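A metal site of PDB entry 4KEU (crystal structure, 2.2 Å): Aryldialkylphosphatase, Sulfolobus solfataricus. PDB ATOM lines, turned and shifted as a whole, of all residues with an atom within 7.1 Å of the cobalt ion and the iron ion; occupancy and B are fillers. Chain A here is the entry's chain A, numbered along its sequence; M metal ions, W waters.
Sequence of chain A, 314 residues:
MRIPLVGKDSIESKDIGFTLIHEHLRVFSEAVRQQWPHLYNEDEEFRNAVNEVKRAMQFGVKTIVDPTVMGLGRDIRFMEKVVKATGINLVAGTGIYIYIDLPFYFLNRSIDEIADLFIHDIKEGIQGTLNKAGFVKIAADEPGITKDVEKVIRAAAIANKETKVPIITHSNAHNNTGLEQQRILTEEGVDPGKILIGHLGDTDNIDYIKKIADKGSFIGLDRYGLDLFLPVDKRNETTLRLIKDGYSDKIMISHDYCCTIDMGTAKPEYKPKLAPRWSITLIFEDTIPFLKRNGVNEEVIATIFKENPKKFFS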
ATOM      1  N   HIS A  22      -7.839  -8.149  23.689  1.00  0.00           N
ATOM      2  CA  HIS A  22      -6.837  -9.208  23.766  1.00  0.00           C
ATOM      3  C   HIS A  22      -6.961 -10.014  25.052  1.00  0.00           C
ATOM      4  O   HIS A  22      -6.325  -9.672  26.116  1.00  0.00           O
ATOM      5  CB  HIS A  22      -5.369  -8.611  23.625  1.00  0.00           C
ATOM      6  CG  HIS A  22      -4.248  -9.708  23.427  1.00  0.00           C
ATOM      7  ND1 HIS A  22      -3.252  -9.596  22.466  1.00  0.00           N
ATOM      8  CD2 HIS A  22      -4.012 -10.930  24.094  1.00  0.00           C
ATOM      9  CE1 HIS A  22      -2.426 -10.679  22.529  1.00  0.00           C
ATOM     10  NE2 HIS A  22      -2.884 -11.504  23.510  1.00  0.00           N
ATOM     11  N   GLU A  23      -7.763 -11.085  24.988  1.00  0.00           N
ATOM     12  CA  GLU A  23      -7.891 -12.017  26.105  1.00  0.00           C
ATOM     13  C   GLU A  23      -7.936 -13.431  25.570  1.00  0.00           C
ATOM     14  O   GLU A  23      -8.369 -13.659  24.459  1.00  0.00           O
ATOM     15  CB  GLU A  23      -9.185 -11.734  26.950  1.00  0.00           C
ATOM     16  CG  GLU A  23      -9.420 -10.250  27.319  1.00  0.00           C
ATOM     17  CD  GLU A  23      -8.415  -9.712  28.341  1.00  0.00           C
ATOM     18  OE1 GLU A  23      -8.248  -8.449  28.404  1.00  0.00           O
ATOM     19  OE2 GLU A  23      -7.778 -10.557  29.110  1.00  0.00           O
ATOM     20  N   HIS A  24      -7.481 -14.399  26.392  1.00  0.00           N
ATOM     21  CA  HIS A  24      -7.514 -15.830  25.994  1.00  0.00           C
ATOM     22  C   HIS A  24      -8.436 -16.641  26.893  1.00  0.00           C
ATOM     23  O   HIS A  24      -8.284 -16.644  28.098  1.00  0.00           O
ATOM     24  CB  HIS A  24      -6.110 -16.432  26.031  1.00  0.00           C
ATOM     25  CG  HIS A  24      -5.081 -15.659  25.209  1.00  0.00           C
ATOM     26  ND1 HIS A  24      -4.852 -15.914  23.881  1.00  0.00           N
ATOM     27  CD2 HIS A  24      -4.191 -14.628  25.559  1.00  0.00           C
ATOM     28  CE1 HIS A  24      -3.883 -15.081  23.419  1.00  0.00           C
ATOM     29  NE2 HIS A  24      -3.477 -14.308  24.424  1.00  0.00           N
ATOM     30  N   VAL A  27      -5.253 -21.386  26.688  1.00  0.00           N
ATOM     31  CA  VAL A  27      -4.049 -21.544  25.904  1.00  0.00           C
ATOM     32  C   VAL A  27      -3.327 -22.856  26.242  1.00  0.00           C
ATOM     33  O   VAL A  27      -3.206 -23.214  27.399  1.00  0.00           O
ATOM     34  CB  VAL A  27      -3.061 -20.351  26.110  1.00  0.00           C
ATOM     35  CG1 VAL A  27      -1.727 -20.662  25.482  1.00  0.00           C
ATOM     36  CG2 VAL A  27      -3.628 -19.080  25.533  1.00  0.00           C
ATOM     37  N   PRO A  67      -7.149 -13.774  20.614  1.00  0.00           N
ATOM     38  CA  PRO A  67      -6.093 -14.075  19.603  1.00  0.00           C
ATOM     39  C   PRO A  67      -5.369 -15.422  19.808  1.00  0.00           C
ATOM     40  O   PRO A  67      -4.162 -15.526  19.535  1.00  0.00           O
ATOM     41  CB  PRO A  67      -5.119 -12.914  19.764  1.00  0.00           C
ATOM     42  CG  PRO A  67      -5.232 -12.518  21.210  1.00  0.00           C
ATOM     43  CD  PRO A  67      -6.651 -12.875  21.670  1.00  0.00           C
ATOM     44  N   THR A  68      -6.085 -16.429  20.278  1.00  0.00           N
ATOM     45  CA  THR A  68      -5.549 -17.779  20.350  1.00  0.00           C
ATOM     46  C   THR A  68      -5.528 -18.385  18.976  1.00  0.00           C
ATOM     47  O   THR A  68      -6.572 -18.507  18.326  1.00  0.00           O
ATOM     48  CB  THR A  68      -6.419 -18.708  21.306  1.00  0.00           C
ATOM     49  OG1 THR A  68      -6.707 -18.027  22.512  1.00  0.00           O
ATOM     50  CG2 THR A  68      -5.697 -19.966  21.624  1.00  0.00           C
ATOM     51  N   LEU A  72      -1.027 -21.727  20.044  1.00  0.00           N
ATOM     52  CA  LEU A  72      -1.601 -21.380  21.342  1.00  0.00           C
ATOM     53  C   LEU A  72      -2.800 -22.276  21.698  1.00  0.00           C
ATOM     54  O   LEU A  72      -3.440 -22.090  22.746  1.00  0.00           O
ATOM     55  CB  LEU A  72      -2.022 -19.872  21.373  1.00  0.00           C
ATOM     56  CG  LEU A  72      -0.855 -18.831  21.216  1.00  0.00           C
ATOM     57  CD1 LEU A  72      -1.383 -17.436  21.096  1.00  0.00           C
ATOM     58  CD2 LEU A  72       0.174 -18.950  22.392  1.00  0.00           C
ATOM     59  N   TYR A  97       1.440 -18.499  15.572  1.00  0.00           N
ATOM     60  CA  TYR A  97       2.158 -17.954  16.661  1.00  0.00           C
ATOM     61  C   TYR A  97       3.455 -18.728  16.857  1.00  0.00           C
ATOM     62  O   TYR A  97       3.441 -19.856  17.381  1.00  0.00           O
ATOM     63  CB  TYR A  97       1.297 -18.027  17.925  1.00  0.00           C
ATOM     64  CG  TYR A  97       1.894 -17.373  19.168  1.00  0.00           C
ATOM     65  CD1 TYR A  97       2.877 -18.015  19.910  1.00  0.00           C
ATOM     66  CD2 TYR A  97       1.436 -16.099  19.602  1.00  0.00           C
ATOM     67  CE1 TYR A  97       3.413 -17.427  21.038  1.00  0.00           C
ATOM     68  CE2 TYR A  97       1.956 -15.512  20.719  1.00  0.00           C
ATOM     69  CZ  TYR A  97       2.950 -16.167  21.446  1.00  0.00           C
ATOM     70  OH  TYR A  97       3.457 -15.585  22.564  1.00  0.00           O
ATOM     71  N   TYR A  99       8.085 -18.082  17.492  1.00  0.00           N
ATOM     72  CA  TYR A  99       9.182 -17.151  17.824  1.00  0.00           C
ATOM     73  C   TYR A  99      10.386 -17.354  16.926  1.00  0.00           C
ATOM     74  O   TYR A  99      11.123 -16.431  16.652  1.00  0.00           O
ATOM     75  CB  TYR A  99       9.605 -17.290  19.296  1.00  0.00           C
ATOM     76  CG  TYR A  99       8.546 -16.859  20.350  1.00  0.00           C
ATOM     77  CD1 TYR A  99       7.370 -16.182  19.967  1.00  0.00           C
ATOM     78  CD2 TYR A  99       8.743 -17.122  21.733  1.00  0.00           C
ATOM     79  CE1 TYR A  99       6.410 -15.790  20.925  1.00  0.00           C
ATOM     80  CE2 TYR A  99       7.807 -16.734  22.692  1.00  0.00           C
ATOM     81  CZ  TYR A  99       6.649 -16.083  22.305  1.00  0.00           C
ATOM     82  OH  TYR A  99       5.729 -15.698  23.259  1.00  0.00           O
ATOM     83  N   KCX A 137      -3.482 -13.072  13.568  1.00  0.00           N
ATOM     84  CA  KCX A 137      -2.559 -12.888  14.661  1.00  0.00           C
ATOM     85  CB  KCX A 137      -3.097 -13.664  15.897  1.00  0.00           C
ATOM     86  CG  KCX A 137      -2.063 -13.787  17.032  1.00  0.00           C
ATOM     87  CD  KCX A 137      -1.894 -12.482  17.777  1.00  0.00           C
ATOM     88  CE  KCX A 137      -0.866 -12.637  18.957  1.00  0.00           C
ATOM     89  NZ  KCX A 137      -1.455 -13.420  20.110  1.00  0.00           N
ATOM     90  C   KCX A 137      -1.173 -13.380  14.243  1.00  0.00           C
ATOM     91  O   KCX A 137      -1.040 -14.431  13.643  1.00  0.00           O
ATOM     92  CX  KCX A 137      -1.001 -13.257  21.400  1.00  0.00           C
ATOM     93  OQ1 KCX A 137      -1.569 -13.986  22.354  1.00  0.00           O
ATOM     94  OQ2 KCX A 137      -0.058 -12.402  21.727  1.00  0.00           O
ATOM     95  N   ILE A 138      -0.148 -12.596  14.566  1.00  0.00           N
ATOM     96  CA  ILE A 138       1.251 -12.971  14.291  1.00  0.00           C
ATOM     97  C   ILE A 138       2.074 -12.578  15.452  1.00  0.00           C
ATOM     98  O   ILE A 138       1.648 -11.771  16.282  1.00  0.00           O
ATOM     99  CB  ILE A 138       1.811 -12.252  13.047  1.00  0.00           C
ATOM    100  CG1 ILE A 138       1.869 -10.748  13.289  1.00  0.00           C
ATOM    101  CG2 ILE A 138       0.961 -12.598  11.801  1.00  0.00           C
ATOM    102  CD1 ILE A 138       2.194  -9.953  12.069  1.00  0.00           C
ATOM    103  N   ALA A 139       3.323 -13.126  15.527  1.00  0.00           N
ATOM    104  CA  ALA A 139       4.171 -12.888  16.700  1.00  0.00           C
ATOM    105  C   ALA A 139       5.661 -12.791  16.383  1.00  0.00           C
ATOM    106  O   ALA A 139       6.122 -13.251  15.347  1.00  0.00           O
ATOM    107  CB  ALA A 139       3.924 -13.992  17.771  1.00  0.00           C
ATOM    108  N   ASP A 141       9.286 -12.376  19.160  1.00  0.00           N
ATOM    109  CA  ASP A 141       9.733 -12.093  20.483  1.00  0.00           C
ATOM    110  C   ASP A 141      11.257 -11.914  20.550  1.00  0.00           C
ATOM    111  O   ASP A 141      11.862 -11.331  19.624  1.00  0.00           O
ATOM    112  CB  ASP A 141       9.243 -13.198  21.479  1.00  0.00           C
ATOM    113  CG  ASP A 141       9.065 -12.663  22.917  1.00  0.00           C
ATOM    114  OD1 ASP A 141      10.070 -12.471  23.614  1.00  0.00           O
ATOM    115  OD2 ASP A 141       7.912 -12.467  23.345  1.00  0.00           O
ATOM    116  N   THR A 169      -0.782  -8.247  16.658  1.00  0.00           N
ATOM    117  CA  THR A 169       0.535  -8.849  16.814  1.00  0.00           C
ATOM    118  C   THR A 169       0.911  -9.076  18.237  1.00  0.00           C
ATOM    119  O   THR A 169       0.376  -8.482  19.129  1.00  0.00           O
ATOM    120  CB  THR A 169       1.676  -7.985  16.118  1.00  0.00           C
ATOM    121  OG1 THR A 169       2.124  -6.959  17.014  1.00  0.00           O
ATOM    122  CG2 THR A 169       1.182  -7.370  14.840  1.00  0.00           C
ATOM    123  N   HIS A 170       1.834  -9.969  18.424  1.00  0.00           N
ATOM    124  CA  HIS A 170       2.494 -10.154  19.631  1.00  0.00           C
ATOM    125  C   HIS A 170       3.879  -9.691  19.411  1.00  0.00           C
ATOM    126  O   HIS A 170       4.492 -10.013  18.394  1.00  0.00           O
ATOM    127  CB  HIS A 170       2.500 -11.675  19.993  1.00  0.00           C
ATOM    128  CG  HIS A 170       3.430 -12.033  21.136  1.00  0.00           C
ATOM    129  ND1 HIS A 170       2.971 -12.450  22.372  1.00  0.00           N
ATOM    130  CD2 HIS A 170       4.851 -12.034  21.221  1.00  0.00           C
ATOM    131  CE1 HIS A 170       4.028 -12.708  23.185  1.00  0.00           C
ATOM    132  NE2 HIS A 170       5.182 -12.452  22.486  1.00  0.00           N
ATOM    133  N   SER A 171       4.412  -8.916  20.328  1.00  0.00           N
ATOM    134  CA  SER A 171       5.818  -8.448  20.197  1.00  0.00           C
ATOM    135  C   SER A 171       6.542  -8.378  21.533  1.00  0.00           C
ATOM    136  O   SER A 171       5.940  -8.499  22.586  1.00  0.00           O
ATOM    137  CB  SER A 171       5.883  -7.093  19.468  1.00  0.00           C
ATOM    138  OG  SER A 171       5.567  -6.056  20.333  1.00  0.00           O
ATOM    139  N   GLY A 198       1.303  -5.316  19.634  1.00  0.00           N
ATOM    140  CA  GLY A 198       0.990  -5.810  20.965  1.00  0.00           C
ATOM    141  C   GLY A 198       2.077  -5.742  22.014  1.00  0.00           C
ATOM    142  O   GLY A 198       3.279  -5.707  21.703  1.00  0.00           O
ATOM    143  N   HIS A 199       1.645  -5.724  23.264  1.00  0.00           N
ATOM    144  CA  HIS A 199       2.523  -5.833  24.424  1.00  0.00           C
ATOM    145  C   HIS A 199       3.471  -4.682  24.587  1.00  0.00           C
ATOM    146  O   HIS A 199       4.498  -4.798  25.278  1.00  0.00           O
ATOM    147  CB  HIS A 199       3.273  -7.184  24.409  1.00  0.00           C
ATOM    148  CG  HIS A 199       2.355  -8.392  24.159  1.00  0.00           C
ATOM    149  ND1 HIS A 199       1.024  -8.407  24.558  1.00  0.00           N
ATOM    150  CD2 HIS A 199       2.602  -9.615  23.553  1.00  0.00           C
ATOM    151  CE1 HIS A 199       0.459  -9.604  24.203  1.00  0.00           C
ATOM    152  NE2 HIS A 199       1.399 -10.346  23.584  1.00  0.00           N
ATOM    153  N   ASP A 222      -1.664  -4.029  26.777  1.00  0.00           N
ATOM    154  CA  ASP A 222      -2.593  -5.125  26.802  1.00  0.00           C
ATOM    155  C   ASP A 222      -2.209  -6.275  27.732  1.00  0.00           C
ATOM    156  O   ASP A 222      -2.746  -7.394  27.602  1.00  0.00           O
ATOM    157  CB  ASP A 222      -2.750  -5.665  25.361  1.00  0.00           C
ATOM    158  CG  ASP A 222      -1.350  -6.018  24.697  1.00  0.00           C
ATOM    159  OD1 ASP A 222      -1.282  -6.080  23.453  1.00  0.00           O
ATOM    160  OD2 ASP A 222      -0.345  -6.211  25.474  1.00  0.00           O
ATOM    161  N   ARG A 223      -1.322  -6.022  28.651  1.00  0.00           N
ATOM    162  CA  ARG A 223      -0.940  -7.078  29.628  1.00  0.00           C
ATOM    163  C   ARG A 223      -1.112  -6.628  31.083  1.00  0.00           C
ATOM    164  O   ARG A 223      -0.313  -7.002  31.984  1.00  0.00           O
ATOM    165  CB  ARG A 223       0.488  -7.581  29.358  1.00  0.00           C
ATOM    166  CG  ARG A 223       0.571  -8.667  28.240  1.00  0.00           C
ATOM    167  CD  ARG A 223       1.996  -8.978  27.858  1.00  0.00           C
ATOM    168  NE  ARG A 223       2.110 -10.316  27.305  1.00  0.00           N
ATOM    169  CZ  ARG A 223       3.260 -10.844  26.823  1.00  0.00           C
ATOM    170  NH1 ARG A 223       4.368 -10.114  26.821  1.00  0.00           N
ATOM    171  NH2 ARG A 223       3.273 -12.085  26.332  1.00  0.00           N
ATOM    172  N   ASP A 256      -4.596  -9.704  28.456  1.00  0.00           N
ATOM    173  CA  ASP A 256      -3.917 -10.886  27.904  1.00  0.00           C
ATOM    174  C   ASP A 256      -4.091 -12.004  28.878  1.00  0.00           C
ATOM    175  O   ASP A 256      -3.204 -12.823  29.075  1.00  0.00           O
ATOM    176  CB  ASP A 256      -2.419 -10.592  27.695  1.00  0.00           C
ATOM    177  CG  ASP A 256      -1.683 -11.663  26.756  1.00  0.00           C
ATOM    178  OD1 ASP A 256      -2.408 -12.418  25.927  1.00  0.00           O
ATOM    179  OD2 ASP A 256      -0.440 -11.741  26.817  1.00  0.00           O
ATOM    180  N   TYR A 257      -5.236 -12.054  29.498  1.00  0.00           N
ATOM    181  CA  TYR A 257      -5.470 -13.005  30.541  1.00  0.00           C
ATOM    182  C   TYR A 257      -5.814 -14.378  30.003  1.00  0.00           C
ATOM    183  O   TYR A 257      -6.558 -14.507  29.017  1.00  0.00           O
ATOM    184  CB  TYR A 257      -6.564 -12.505  31.503  1.00  0.00           C
ATOM    185  CG  TYR A 257      -6.758 -13.400  32.639  1.00  0.00           C
ATOM    186  CD1 TYR A 257      -7.880 -14.251  32.703  1.00  0.00           C
ATOM    187  CD2 TYR A 257      -5.833 -13.440  33.696  1.00  0.00           C
ATOM    188  CE1 TYR A 257      -8.071 -15.111  33.781  1.00  0.00           C
ATOM    189  CE2 TYR A 257      -6.008 -14.299  34.786  1.00  0.00           C
ATOM    190  CZ  TYR A 257      -7.126 -15.127  34.827  1.00  0.00           C
ATOM    191  OH  TYR A 257      -7.302 -15.972  35.883  1.00  0.00           O
ATOM    192  N   CYS A 258      -5.274 -15.390  30.647  1.00  0.00           N
ATOM    193  CA  CYS A 258      -5.547 -16.750  30.280  1.00  0.00           C
ATOM    194  C   CYS A 258      -6.354 -17.411  31.332  1.00  0.00           C
ATOM    195  O   CYS A 258      -5.820 -17.818  32.358  1.00  0.00           O
ATOM    196  CB  CYS A 258      -4.238 -17.510  30.089  1.00  0.00           C
ATOM    197  SG  CYS A 258      -3.073 -16.690  29.047  1.00  0.00           S
HETATM  198 CO    CO M   1       1.182 -12.177  23.112  1.00  0.00          CO
HETATM  199 FE    FE M   2      -1.952 -13.166  24.113  1.00  0.00          FE
HETATM  200  O   HOH W   1      -0.065 -12.665  24.608  1.00  0.00           O
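NE2 of His 24 is bound to the iron ion. The iron ion is bound by OQ1 of KCX 137 (2.0 Å). The iron ion is bound by NE2 of His 22. Water W1 is bound to the iron ion (2.0 Å). OD1 of Asp 256 is bound to the iron ion.
OQ2 of KCX 137 is bound to the cobalt ion, 1.9 Å away. NE2 of His 199 binds the cobalt ion (1.9 Å). A ring nitrogen (ND1) of His 170 binds the cobalt ion (2.0 Å). Water W1 is bound to the cobalt ion, at 2.0 Å.
The backbone NH of His 24 lies within hydrogen-bond range of the backbone carbonyl oxygen of Tyr 257, 2.8 Å away. The backbone NH of Asp 256 is in hydrogen-bond range of the side-chain carboxylate of Glu 23, 3.4 Å away. NE2 of His 170 sits at hydrogen-bond distance from OD2 of Asp 141 (2.9 Å). The guanidinium group (NE) of Arg 223 is in salt-bridge range of the side-chain carboxylate (OD2) of Asp 256 (3.0 Å). A ring nitrogen (ND1) of His 24 sits at hydrogen-bond distance from the side-chain hydroxyl (OG1) of Thr 68, at 3.1 Å. ND1 of His 199 sits at hydrogen-bond distance from OD2 of Asp 222, 2.7 Å away. The backbone NH (N) of His 170 lies within hydrogen-bond range of the backbone carbonyl oxygen (O) of Ile 138 (2.8 Å). The backbone carbonyl oxygen (O) of Pro 67 sits at hydrogen-bond distance from NZ of KCX 137 (3.5 Å).
Residues that only touch the cobalt ion: Arg 223. The nearest printed residue that does not touch the cobalt ion is Asp 256 (4.1 Å).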
